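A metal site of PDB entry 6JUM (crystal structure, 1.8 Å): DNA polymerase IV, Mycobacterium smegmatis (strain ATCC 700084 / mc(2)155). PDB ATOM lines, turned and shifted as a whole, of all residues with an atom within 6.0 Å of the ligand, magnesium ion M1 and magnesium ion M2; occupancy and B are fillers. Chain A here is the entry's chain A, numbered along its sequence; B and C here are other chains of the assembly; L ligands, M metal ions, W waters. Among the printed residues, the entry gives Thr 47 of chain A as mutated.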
ATOM      1  N   HIS A   7     -10.502  18.782   2.098  1.00  0.00           N
ATOM      2  CA  HIS A   7      -9.672  17.725   2.481  1.00  0.00           C
ATOM      3  C   HIS A   7      -8.251  18.290   2.742  1.00  0.00           C
ATOM      4  O   HIS A   7      -7.782  18.998   1.907  1.00  0.00           O
ATOM      5  CB  HIS A   7      -9.509  16.725   1.393  1.00  0.00           C
ATOM      6  CG  HIS A   7      -8.573  15.610   1.756  1.00  0.00           C
ATOM      7  ND1 HIS A   7      -7.302  15.533   1.264  1.00  0.00           N
ATOM      8  CD2 HIS A   7      -8.698  14.577   2.635  1.00  0.00           C
ATOM      9  CE1 HIS A   7      -6.700  14.461   1.740  1.00  0.00           C
ATOM     10  NE2 HIS A   7      -7.506  13.864   2.590  1.00  0.00           N
ATOM     11  N   ASP A   9      -4.288  17.837   3.943  1.00  0.00           N
ATOM     12  CA  ASP A   9      -3.238  16.798   3.917  1.00  0.00           C
ATOM     13  C   ASP A   9      -1.875  17.474   4.112  1.00  0.00           C
ATOM     14  O   ASP A   9      -1.521  18.391   3.403  1.00  0.00           O
ATOM     15  CB  ASP A   9      -3.198  15.860   2.632  1.00  0.00           C
ATOM     16  CG  ASP A   9      -2.253  14.758   2.783  1.00  0.00           C
ATOM     17  OD1 ASP A   9      -1.186  15.166   2.712  1.00  0.00           O
ATOM     18  OD2 ASP A   9      -2.483  13.582   3.002  1.00  0.00           O
ATOM     19  N   LEU A  10      -1.216  17.039   5.219  1.00  0.00           N
ATOM     20  CA  LEU A  10       0.166  17.560   5.549  1.00  0.00           C
ATOM     21  C   LEU A  10       1.169  17.298   4.432  1.00  0.00           C
ATOM     22  O   LEU A  10       1.320  16.263   3.906  1.00  0.00           O
ATOM     23  CB  LEU A  10       0.593  16.974   6.947  1.00  0.00           C
ATOM     24  CG  LEU A  10      -0.234  17.541   8.128  1.00  0.00           C
ATOM     25  CD1 LEU A  10      -0.008  16.785   9.412  1.00  0.00           C
ATOM     26  CD2 LEU A  10       0.101  18.999   8.350  1.00  0.00           C
ATOM     27  N   ASP A  11       1.873  18.327   4.049  1.00  0.00           N
ATOM     28  CA  ASP A  11       2.976  18.202   3.062  1.00  0.00           C
ATOM     29  C   ASP A  11       4.183  17.470   3.578  1.00  0.00           C
ATOM     30  O   ASP A  11       4.659  17.734   4.742  1.00  0.00           O
ATOM     31  CB  ASP A  11       3.429  19.606   2.558  1.00  0.00           C
ATOM     32  CG  ASP A  11       2.401  20.336   1.803  1.00  0.00           C
ATOM     33  OD1 ASP A  11       1.218  19.776   1.551  1.00  0.00           O
ATOM     34  OD2 ASP A  11       2.650  21.581   1.584  1.00  0.00           O
ATOM     35  N   GLN A  12       4.667  16.549   2.732  1.00  0.00           N
ATOM     36  CA  GLN A  12       5.843  15.754   3.095  1.00  0.00           C
ATOM     37  C   GLN A  12       6.000  15.510   4.656  1.00  0.00           C
ATOM     38  O   GLN A  12       7.017  15.785   5.238  1.00  0.00           O
ATOM     39  CB  GLN A  12       7.093  16.383   2.477  1.00  0.00           C
ATOM     40  CG  GLN A  12       7.353  17.860   2.812  1.00  0.00           C
ATOM     41  CD  GLN A  12       8.619  18.433   2.191  1.00  0.00           C
ATOM     42  OE1 GLN A  12       9.359  17.758   1.463  1.00  0.00           O
ATOM     43  NE2 GLN A  12       8.720  19.719   2.249  1.00  0.00           N
ATOM     44  N   PHE A  13       4.982  14.882   5.220  1.00  0.00           N
ATOM     45  CA  PHE A  13       4.719  14.988   6.746  1.00  0.00           C
ATOM     46  C   PHE A  13       5.931  14.761   7.593  1.00  0.00           C
ATOM     47  O   PHE A  13       6.379  15.669   8.294  1.00  0.00           O
ATOM     48  CB  PHE A  13       3.585  14.011   7.140  1.00  0.00           C
ATOM     49  CG  PHE A  13       3.252  13.969   8.588  1.00  0.00           C
ATOM     50  CD1 PHE A  13       3.234  15.095   9.308  1.00  0.00           C
ATOM     51  CD2 PHE A  13       2.841  12.819   9.147  1.00  0.00           C
ATOM     52  CE1 PHE A  13       2.963  15.099  10.689  1.00  0.00           C
ATOM     53  CE2 PHE A  13       2.572  12.762  10.521  1.00  0.00           C
ATOM     54  CZ  PHE A  13       2.542  13.952  11.250  1.00  0.00           C
ATOM     55  N   LEU A  14       6.461  13.557   7.538  1.00  0.00           N
ATOM     56  CA  LEU A  14       7.608  13.251   8.429  1.00  0.00           C
ATOM     57  C   LEU A  14       8.818  14.138   8.153  1.00  0.00           C
ATOM     58  O   LEU A  14       9.463  14.553   9.125  1.00  0.00           O
ATOM     59  CB  LEU A  14       7.958  11.809   8.346  1.00  0.00           C
ATOM     60  CG  LEU A  14       7.089  10.742   9.037  1.00  0.00           C
ATOM     61  CD1 LEU A  14       5.668  10.959   9.253  1.00  0.00           C
ATOM     62  CD2 LEU A  14       7.368   9.301   8.737  1.00  0.00           C
ATOM     63  N   ALA A  15       9.105  14.480   6.881  1.00  0.00           N
ATOM     64  CA  ALA A  15      10.194  15.467   6.556  1.00  0.00           C
ATOM     65  C   ALA A  15       9.929  16.857   7.126  1.00  0.00           C
ATOM     66  O   ALA A  15      10.862  17.481   7.650  1.00  0.00           O
ATOM     67  CB  ALA A  15      10.482  15.633   5.087  1.00  0.00           C
ATOM     68  N   VAL A  45      12.967   3.955   2.984  1.00  0.00           N
ATOM     69  CA  VAL A  45      12.500   5.309   3.081  1.00  0.00           C
ATOM     70  C   VAL A  45      11.059   5.304   3.631  1.00  0.00           C
ATOM     71  O   VAL A  45      10.217   4.628   3.104  1.00  0.00           O
ATOM     72  CB  VAL A  45      12.505   6.008   1.714  1.00  0.00           C
ATOM     73  CG1 VAL A  45      11.897   7.404   1.747  1.00  0.00           C
ATOM     74  CG2 VAL A  45      13.914   6.100   1.153  1.00  0.00           C
ATOM     75  N   THR A  46      10.824   6.027   4.697  1.00  0.00           N
ATOM     76  CA  THR A  46       9.471   6.353   5.122  1.00  0.00           C
ATOM     77  C   THR A  46       8.968   7.650   4.521  1.00  0.00           C
ATOM     78  O   THR A  46       7.831   7.684   4.110  1.00  0.00           O
ATOM     79  CB  THR A  46       9.345   6.286   6.718  1.00  0.00           C
ATOM     80  OG1 THR A  46       8.029   6.748   7.092  1.00  0.00           O
ATOM     81  CG2 THR A  46      10.144   7.227   7.335  1.00  0.00           C
ATOM     82  N   THR A  47       9.778   8.678   4.464  1.00  0.00           N
ATOM     83  CA  THR A  47       9.377   9.886   3.723  1.00  0.00           C
ATOM     84  C   THR A  47      10.597  10.520   3.060  1.00  0.00           C
ATOM     85  O   THR A  47      11.587  10.704   3.677  1.00  0.00           O
ATOM     86  CB  THR A  47       8.800  10.992   4.677  1.00  0.00           C
ATOM     87  OG1 THR A  47       7.686  10.528   5.457  1.00  0.00           O
ATOM     88  CG2 THR A  47       8.374  12.350   3.920  1.00  0.00           C
ATOM     89  N   ALA A  48      10.533  10.830   1.775  1.00  0.00           N
ATOM     90  CA  ALA A  48      11.473  11.678   1.111  1.00  0.00           C
ATOM     91  C   ALA A  48      10.888  13.106   0.971  1.00  0.00           C
ATOM     92  O   ALA A  48       9.681  13.224   0.707  1.00  0.00           O
ATOM     93  CB  ALA A  48      11.736  11.186  -0.307  1.00  0.00           C
ATOM     94  N   TYR A  50      10.295  16.684  -0.812  1.00  0.00           N
ATOM     95  CA  TYR A  50       9.960  16.910  -2.197  1.00  0.00           C
ATOM     96  C   TYR A  50      11.266  17.018  -3.050  1.00  0.00           C
ATOM     97  O   TYR A  50      11.242  16.660  -4.256  1.00  0.00           O
ATOM     98  CB  TYR A  50       9.208  18.213  -2.311  1.00  0.00           C
ATOM     99  CG  TYR A  50       7.815  18.171  -1.740  1.00  0.00           C
ATOM    100  CD1 TYR A  50       7.012  17.108  -1.843  1.00  0.00           C
ATOM    101  CD2 TYR A  50       7.331  19.229  -1.018  1.00  0.00           C
ATOM    102  CE1 TYR A  50       5.676  17.094  -1.291  1.00  0.00           C
ATOM    103  CE2 TYR A  50       6.049  19.251  -0.553  1.00  0.00           C
ATOM    104  CZ  TYR A  50       5.239  18.172  -0.667  1.00  0.00           C
ATOM    105  OH  TYR A  50       3.941  18.331  -0.165  1.00  0.00           O
ATOM    106  N   ARG A  53      12.396  13.568  -3.847  1.00  0.00           N
ATOM    107  CA  ARG A  53      11.472  12.987  -4.757  1.00  0.00           C
ATOM    108  C   ARG A  53      11.782  13.323  -6.205  1.00  0.00           C
ATOM    109  O   ARG A  53      11.507  12.529  -7.087  1.00  0.00           O
ATOM    110  CB  ARG A  53      10.010  13.443  -4.506  1.00  0.00           C
ATOM    111  CG  ARG A  53       9.484  12.881  -3.212  1.00  0.00           C
ATOM    112  CD  ARG A  53       7.978  13.227  -2.829  1.00  0.00           C
ATOM    113  NE  ARG A  53       7.814  13.132  -1.411  1.00  0.00           N
ATOM    114  CZ  ARG A  53       6.599  13.196  -0.844  1.00  0.00           C
ATOM    115  NH1 ARG A  53       5.528  13.422  -1.537  1.00  0.00           N
ATOM    116  NH2 ARG A  53       6.501  13.102   0.438  1.00  0.00           N
ATOM    117  N   ALA A  59       8.668   6.715  -0.755  1.00  0.00           N
ATOM    118  CA  ALA A  59       8.411   5.854   0.408  1.00  0.00           C
ATOM    119  C   ALA A  59       8.497   4.368  -0.079  1.00  0.00           C
ATOM    120  O   ALA A  59       8.045   4.049  -1.160  1.00  0.00           O
ATOM    121  CB  ALA A  59       6.973   6.142   0.980  1.00  0.00           C
ATOM    122  N   GLY A  60       9.058   3.486   0.728  1.00  0.00           N
ATOM    123  CA  GLY A  60       9.288   2.067   0.371  1.00  0.00           C
ATOM    124  C   GLY A  60      10.601   1.699  -0.230  1.00  0.00           C
ATOM    125  O   GLY A  60      10.945   0.532  -0.352  1.00  0.00           O
ATOM    126  N   TRP A 106      -3.223   9.443  10.028  1.00  0.00           N
ATOM    127  CA  TRP A 106      -2.275  10.250  10.669  1.00  0.00           C
ATOM    128  C   TRP A 106      -2.125  11.709  10.261  1.00  0.00           C
ATOM    129  O   TRP A 106      -1.835  12.605  11.080  1.00  0.00           O
ATOM    130  CB  TRP A 106      -0.998   9.479  10.226  1.00  0.00           C
ATOM    131  CG  TRP A 106      -0.045   9.515  11.193  1.00  0.00           C
ATOM    132  CD1 TRP A 106      -0.153   9.925  12.463  1.00  0.00           C
ATOM    133  CD2 TRP A 106       1.251   9.077  10.983  1.00  0.00           C
ATOM    134  NE1 TRP A 106       1.101   9.785  13.101  1.00  0.00           N
ATOM    135  CE2 TRP A 106       1.973   9.259  12.205  1.00  0.00           C
ATOM    136  CE3 TRP A 106       1.917   8.593   9.878  1.00  0.00           C
ATOM    137  CZ2 TRP A 106       3.310   8.913  12.341  1.00  0.00           C
ATOM    138  CZ3 TRP A 106       3.257   8.249  10.028  1.00  0.00           C
ATOM    139  CH2 TRP A 106       3.944   8.429  11.237  1.00  0.00           C
ATOM    140  N   ASP A 107      -2.228  11.955   8.981  1.00  0.00           N
ATOM    141  CA  ASP A 107      -1.805  13.258   8.419  1.00  0.00           C
ATOM    142  C   ASP A 107      -2.906  13.986   7.580  1.00  0.00           C
ATOM    143  O   ASP A 107      -2.664  15.005   6.908  1.00  0.00           O
ATOM    144  CB  ASP A 107      -0.462  13.104   7.639  1.00  0.00           C
ATOM    145  CG  ASP A 107      -0.576  13.069   6.100  1.00  0.00           C
ATOM    146  OD1 ASP A 107      -1.429  12.293   5.650  1.00  0.00           O
ATOM    147  OD2 ASP A 107       0.142  13.780   5.419  1.00  0.00           O
ATOM    148  N   GLU A 108      -4.172  13.522   7.691  1.00  0.00           N
ATOM    149  CA  GLU A 108      -5.167  14.164   6.910  1.00  0.00           C
ATOM    150  C   GLU A 108      -6.515  14.162   7.582  1.00  0.00           C
ATOM    151  O   GLU A 108      -6.791  13.282   8.449  1.00  0.00           O
ATOM    152  CB  GLU A 108      -5.279  13.585   5.539  1.00  0.00           C
ATOM    153  CG  GLU A 108      -5.444  12.103   5.393  1.00  0.00           C
ATOM    154  CD  GLU A 108      -5.153  11.635   3.978  1.00  0.00           C
ATOM    155  OE1 GLU A 108      -4.137  11.019   3.737  1.00  0.00           O
ATOM    156  OE2 GLU A 108      -6.131  11.541   3.204  1.00  0.00           O
ATOM    157  N   LYS A 152     -10.480  14.723  -2.084  1.00  0.00           N
ATOM    158  CA  LYS A 152      -9.211  14.027  -1.997  1.00  0.00           C
ATOM    159  C   LYS A 152      -8.459  14.044  -3.302  1.00  0.00           C
ATOM    160  O   LYS A 152      -7.228  14.309  -3.271  1.00  0.00           O
ATOM    161  CB  LYS A 152      -9.470  12.553  -1.535  1.00  0.00           C
ATOM    162  CG  LYS A 152      -8.270  11.634  -1.567  1.00  0.00           C
ATOM    163  CD  LYS A 152      -7.196  11.985  -0.553  1.00  0.00           C
ATOM    164  CE  LYS A 152      -6.386  10.685  -0.328  1.00  0.00           C
ATOM    165  NZ  LYS A 152      -5.178  11.070   0.534  1.00  0.00           N
ATOM    166  N   LYS A 159      -1.220  20.072  -4.182  1.00  0.00           N
ATOM    167  CA  LYS A 159       0.151  19.889  -3.724  1.00  0.00           C
ATOM    168  C   LYS A 159       1.150  20.542  -4.686  1.00  0.00           C
ATOM    169  O   LYS A 159       0.904  20.414  -5.895  1.00  0.00           O
ATOM    170  CB  LYS A 159       0.468  18.431  -3.744  1.00  0.00           C
ATOM    171  CG  LYS A 159      -0.194  17.609  -2.678  1.00  0.00           C
ATOM    172  CD  LYS A 159       0.152  17.944  -1.289  1.00  0.00           C
ATOM    173  CE  LYS A 159      -0.462  16.946  -0.263  1.00  0.00           C
ATOM    174  NZ  LYS A 159       0.272  17.185   1.036  1.00  0.00           N
ATOM    175  P    DC B  18      -3.287   7.415   0.110  1.00  0.00           P
ATOM    176  OP1  DC B  18      -3.882   8.778  -0.136  1.00  0.00           O
ATOM    177  OP2  DC B  18      -2.171   7.093  -0.807  1.00  0.00           O
ATOM    178  O5'  DC B  18      -2.735   7.231   1.556  1.00  0.00           O
ATOM    179  C5'  DC B  18      -3.526   7.592   2.640  1.00  0.00           C
ATOM    180  C4'  DC B  18      -2.710   7.514   3.896  1.00  0.00           C
ATOM    181  O4'  DC B  18      -2.452   6.127   4.185  1.00  0.00           O
ATOM    182  C3'  DC B  18      -1.347   8.188   3.906  1.00  0.00           C
ATOM    183  O3'  DC B  18      -1.442   9.513   4.463  1.00  0.00           O
ATOM    184  C2'  DC B  18      -0.595   7.383   4.946  1.00  0.00           C
ATOM    185  C1'  DC B  18      -1.126   5.986   4.723  1.00  0.00           C
ATOM    186  N1   DC B  18      -0.339   5.009   3.878  1.00  0.00           N
ATOM    187  C2   DC B  18       0.547   4.166   4.570  1.00  0.00           C
ATOM    188  O2   DC B  18       0.769   4.402   5.770  1.00  0.00           O
ATOM    189  N3   DC B  18       1.179   3.174   3.902  1.00  0.00           N
ATOM    190  C4   DC B  18       0.939   2.983   2.612  1.00  0.00           C
ATOM    191  N4   DC B  18       1.579   1.971   2.005  1.00  0.00           N
ATOM    192  C5   DC B  18       0.042   3.825   1.872  1.00  0.00           C
ATOM    193  C6   DC B  18      -0.592   4.799   2.550  1.00  0.00           C
ATOM    194  P    DG C   4      11.136  -5.018   2.965  1.00  0.00           P
ATOM    195  OP1  DG C   4      11.880  -6.167   3.554  1.00  0.00           O
ATOM    196  OP2  DG C   4       9.703  -5.192   2.538  1.00  0.00           O
ATOM    197  O5'  DG C   4      11.110  -3.844   4.013  1.00  0.00           O
ATOM    198  C5'  DG C   4      12.203  -3.467   4.848  1.00  0.00           C
ATOM    199  C4'  DG C   4      11.625  -2.802   6.066  1.00  0.00           C
ATOM    200  O4'  DG C   4      10.978  -1.548   5.731  1.00  0.00           O
ATOM    201  C3'  DG C   4      10.584  -3.647   6.845  1.00  0.00           C
ATOM    202  O3'  DG C   4      10.783  -3.472   8.260  1.00  0.00           O
ATOM    203  C2'  DG C   4       9.265  -3.104   6.358  1.00  0.00           C
ATOM    204  C1'  DG C   4       9.583  -1.614   6.040  1.00  0.00           C
ATOM    205  N9   DG C   4       8.839  -1.051   4.915  1.00  0.00           N
ATOM    206  C8   DG C   4       8.724  -1.577   3.655  1.00  0.00           C
ATOM    207  N7   DG C   4       8.017  -0.837   2.850  1.00  0.00           N
ATOM    208  C5   DG C   4       7.576   0.209   3.635  1.00  0.00           C
ATOM    209  C6   DG C   4       6.746   1.325   3.318  1.00  0.00           C
ATOM    210  O6   DG C   4       6.267   1.632   2.226  1.00  0.00           O
ATOM    211  N1   DG C   4       6.595   2.180   4.402  1.00  0.00           N
ATOM    212  C2   DG C   4       7.103   1.947   5.667  1.00  0.00           C
ATOM    213  N2   DG C   4       6.811   2.840   6.598  1.00  0.00           N
ATOM    214  N3   DG C   4       7.864   0.897   5.972  1.00  0.00           N
ATOM    215  C4   DG C   4       8.045   0.074   4.934  1.00  0.00           C
ATOM    216  P    DG C   5       9.814  -4.272   9.301  1.00  0.00           P
ATOM    217  OP1  DG C   5      10.588  -4.329  10.536  1.00  0.00           O
ATOM    218  OP2  DG C   5       9.110  -5.364   8.636  1.00  0.00           O
ATOM    219  O5'  DG C   5       8.596  -3.242   9.447  1.00  0.00           O
ATOM    220  C5'  DG C   5       8.866  -2.019  10.143  1.00  0.00           C
ATOM    221  C4'  DG C   5       7.545  -1.295  10.309  1.00  0.00           C
ATOM    222  O4'  DG C   5       7.069  -0.840   9.003  1.00  0.00           O
ATOM    223  C3'  DG C   5       6.406  -2.154  10.910  1.00  0.00           C
ATOM    224  O3'  DG C   5       5.749  -1.379  11.926  1.00  0.00           O
ATOM    225  C2'  DG C   5       5.452  -2.373   9.741  1.00  0.00           C
ATOM    226  C1'  DG C   5       5.655  -1.077   8.972  1.00  0.00           C
ATOM    227  N9   DG C   5       5.243  -1.079   7.575  1.00  0.00           N
ATOM    228  C8   DG C   5       5.548  -2.000   6.600  1.00  0.00           C
ATOM    229  N7   DG C   5       5.086  -1.683   5.428  1.00  0.00           N
ATOM    230  C5   DG C   5       4.362  -0.516   5.659  1.00  0.00           C
ATOM    231  C6   DG C   5       3.615   0.298   4.772  1.00  0.00           C
ATOM    232  O6   DG C   5       3.384   0.102   3.576  1.00  0.00           O
ATOM    233  N1   DG C   5       3.072   1.398   5.414  1.00  0.00           N
ATOM    234  C2   DG C   5       3.247   1.714   6.733  1.00  0.00           C
ATOM    235  N2   DG C   5       2.638   2.848   7.182  1.00  0.00           N
ATOM    236  N3   DG C   5       3.936   0.956   7.576  1.00  0.00           N
ATOM    237  C4   DG C   5       4.509  -0.100   6.963  1.00  0.00           C
HETATM  238  P1  LIG L   1       2.447  14.516   0.541  1.00  0.00           P
HETATM  239  O1  LIG L   1       2.599  14.087  -0.879  1.00  0.00           O
HETATM  240  O2  LIG L   1       1.114  14.086   1.204  1.00  0.00           O
HETATM  241  O3  LIG L   1       2.878  15.890   0.542  1.00  0.00           O
HETATM  242  P2  LIG L   1       3.493  12.691   2.604  1.00  0.00           P
HETATM  243  O4  LIG L   1       4.990  12.426   2.878  1.00  0.00           O
HETATM  244  O5  LIG L   1       2.870  13.414   3.693  1.00  0.00           O
HETATM  245  O6  LIG L   1       3.564  13.606   1.350  1.00  0.00           O
HETATM  246  P3  LIG L   1       1.143  10.825   2.589  1.00  0.00           P
HETATM  247  O7  LIG L   1       0.309  11.897   3.158  1.00  0.00           O
HETATM  248  O8  LIG L   1       0.665   9.793   1.581  1.00  0.00           O
HETATM  249  N1  LIG L   1       2.562  11.425   2.092  1.00  0.00           N
HETATM  250  O9  LIG L   1       1.383   9.843   3.799  1.00  0.00           O
HETATM  251  C1  LIG L   1       1.765  10.391   5.080  1.00  0.00           C
HETATM  252  C2  LIG L   1       2.955   9.786   5.833  1.00  0.00           C
HETATM  253  O10 LIG L   1       2.571   8.378   6.038  1.00  0.00           O
HETATM  254  C3  LIG L   1       4.223   9.840   5.212  1.00  0.00           C
HETATM  255  O11 LIG L   1       4.958  11.112   5.318  1.00  0.00           O
HETATM  256  C4  LIG L   1       4.881   8.572   5.990  1.00  0.00           C
HETATM  257  C5  LIG L   1       3.855   7.594   6.112  1.00  0.00           C
HETATM  258  N2  LIG L   1       3.817   6.676   4.977  1.00  0.00           N
HETATM  259  C6  LIG L   1       4.646   5.382   5.181  1.00  0.00           C
HETATM  260  N3  LIG L   1       4.720   4.459   4.076  1.00  0.00           N
HETATM  261  C7  LIG L   1       4.074   4.697   2.854  1.00  0.00           C
HETATM  262  C8  LIG L   1       3.302   5.975   2.637  1.00  0.00           C
HETATM  263  C9  LIG L   1       3.137   6.906   3.750  1.00  0.00           C
HETATM  264  O12 LIG L   1       5.247   5.245   6.267  1.00  0.00           O
HETATM  265  N4  LIG L   1       4.245   3.796   1.823  1.00  0.00           N
HETATM  266 MG    MG M   1       0.701  14.076   3.386  1.00  0.00          MG
HETATM  267 MG    MG M   2      -1.916  11.615   3.595  1.00  0.00          MG
HETATM  268  O   HOH W   1       0.709   7.167   0.452  1.00  0.00           O
HETATM  269  O   HOH W   2      -0.921  12.911   0.028  1.00  0.00           O
HETATM  270  O   HOH W   3      -1.920  10.768   1.347  1.00  0.00           O
HETATM  271  O   HOH W   4       2.780  15.408  -3.331  1.00  0.00           O
HETATM  272  O   HOH W   5       3.162   4.262  -0.964  1.00  0.00           O
HETATM  273  O   HOH W   6       3.959   9.146   0.779  1.00  0.00           O
HETATM  274  O   HOH W   7       6.072   9.418   2.443  1.00  0.00           O
HETATM  275  O   HOH W   8       5.067   5.386   8.867  1.00  0.00           O
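The backbone carbonyl oxygen (O) of Asp 9 lies within hydrogen-bond range of the side-chain amino group (NZ) of Lys 159 (3.2 Å).
OE2 of Glu 108 lies within salt-bridge range of NZ of Lys 152, 2.9 Å away.
The side-chain carboxylate (OE2) of Glu 108 is in hydrogen-bond range of a ring nitrogen (NE2) of His 7 (2.8 Å).
OP1 of DC 18 of chain B lies within salt-bridge range of the side-chain amino group of Lys 152 (2.7 Å).
The side-chain amino group of Lys 159 sits close to the backbone carbonyl oxygen of Leu 10, at 3.2 Å.
The side-chain amide oxygen of Gln 12 lies within hydrogen-bond range of the backbone NH of Tyr 50.
The backbone carbonyl oxygen of Ala 48 lies within hydrogen-bond range of the guanidinium group of Arg 53, at 2.8 Å.
The side-chain carboxylate of Asp 11 is in salt-bridge range of the side-chain amino group of Lys 159, at 2.8 Å.
Asp 11 touches the ligand (CA to O3, 3.4 Å).
N of Leu 14 touches O11 of the ligand (3.6 Å).
Ala 59 touches the ligand (CB to N4, 3.7 Å).
CE3 of Trp 106 touches O10 of the ligand, 3.9 Å away.
N2 of DG 5 of chain C touches O12 of the ligand (3.7 Å).
Hydrophobic or aromatic side chains that line the ligand: Phe 13, Leu 14, Tyr 50, Ala 59 and Trp 106.
Lys 159 touches magnesium ion M1.
Within 4 Å of magnesium ion M1: Asp 9, Leu 10, Asp 107 and Lys 159.
The nearest printed residue that does not touch magnesium ion M1 is Asp 11 (4.5 Å).
N4 of DC 18 of chain B lies within hydrogen-bond range of a nitrogen (N4) of the ligand (3.2 Å).
OH of Tyr 50 sits at hydrogen-bond distance from O3 of the ligand (2.8 Å).
An oxygen (O11) of the ligand is in hydrogen-bond range of the side-chain hydroxyl (OG1) of Thr 47 (2.8 Å).
N4 of the ligand sits at hydrogen-bond distance from O6 of DG 4 of chain C (3.0 Å).
The backbone NH of Gln 12 lies within hydrogen-bond range of an oxygen (O3) of the ligand (2.9 Å).
NH2 of Arg 53 lies within salt-bridge range of O4 of the ligand, at 2.9 Å.
The side-chain amino group (NZ) of Lys 159 lies within salt-bridge range of an oxygen (O3) of the ligand.
The backbone NH (N) of Phe 13 is in hydrogen-bond range of an oxygen (O4) of the ligand (3.4 Å).
The side-chain hydroxyl (OG1) of Thr 46 is in hydrogen-bond range of an oxygen (O12) of the ligand, 3.3 Å away.
OD2 of Asp 107 is bound to magnesium ion M1 (2.1 Å).
Magnesium ion M1 is bound by an oxygen (O2) of the ligand (2.2 Å).
O7 of the ligand binds magnesium ion M1 (2.2 Å).
OD1 of Asp 9 is bound to magnesium ion M1.
Magnesium ion M1 is bound by O5 of the ligand.
O of Leu 10 is bound to magnesium ion M1 (2.3 Å).
Magnesium ion M1 has six donor atoms within binding distance.
Magnesium ion M2 is bound by OD2 of Asp 9 (2.1 Å).
OD1 of Asp 107 is bound to magnesium ion M2 (2.2 Å).
Magnesium ion M2 is bound by O7 of the ligand (2.3 Å).
OE1 of Glu 108 binds magnesium ion M2, at 2.3 Å.
O3' of DC 18 of chain B is bound to magnesium ion M2 (2.3 Å).
Magnesium ion M2 is bound by water W3 (2.4 Å).
Magnesium ion M2 has six donor atoms within binding distance.
Water W3 lies within hydrogen-bond range of O8 of the ligand (2.8 Å), OP1 of DC 18 of chain B (3.2 Å) and NZ of Lys 152 (3.4 Å).
Water W1 bridges O8 of the ligand (2.9 Å) and OP2 of DC 18 of chain B (3.1 Å).
Water W7 bridges the backbone carbonyl oxygen of Thr 46 (3.0 Å) and an oxygen (O4) of the ligand (3.2 Å).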
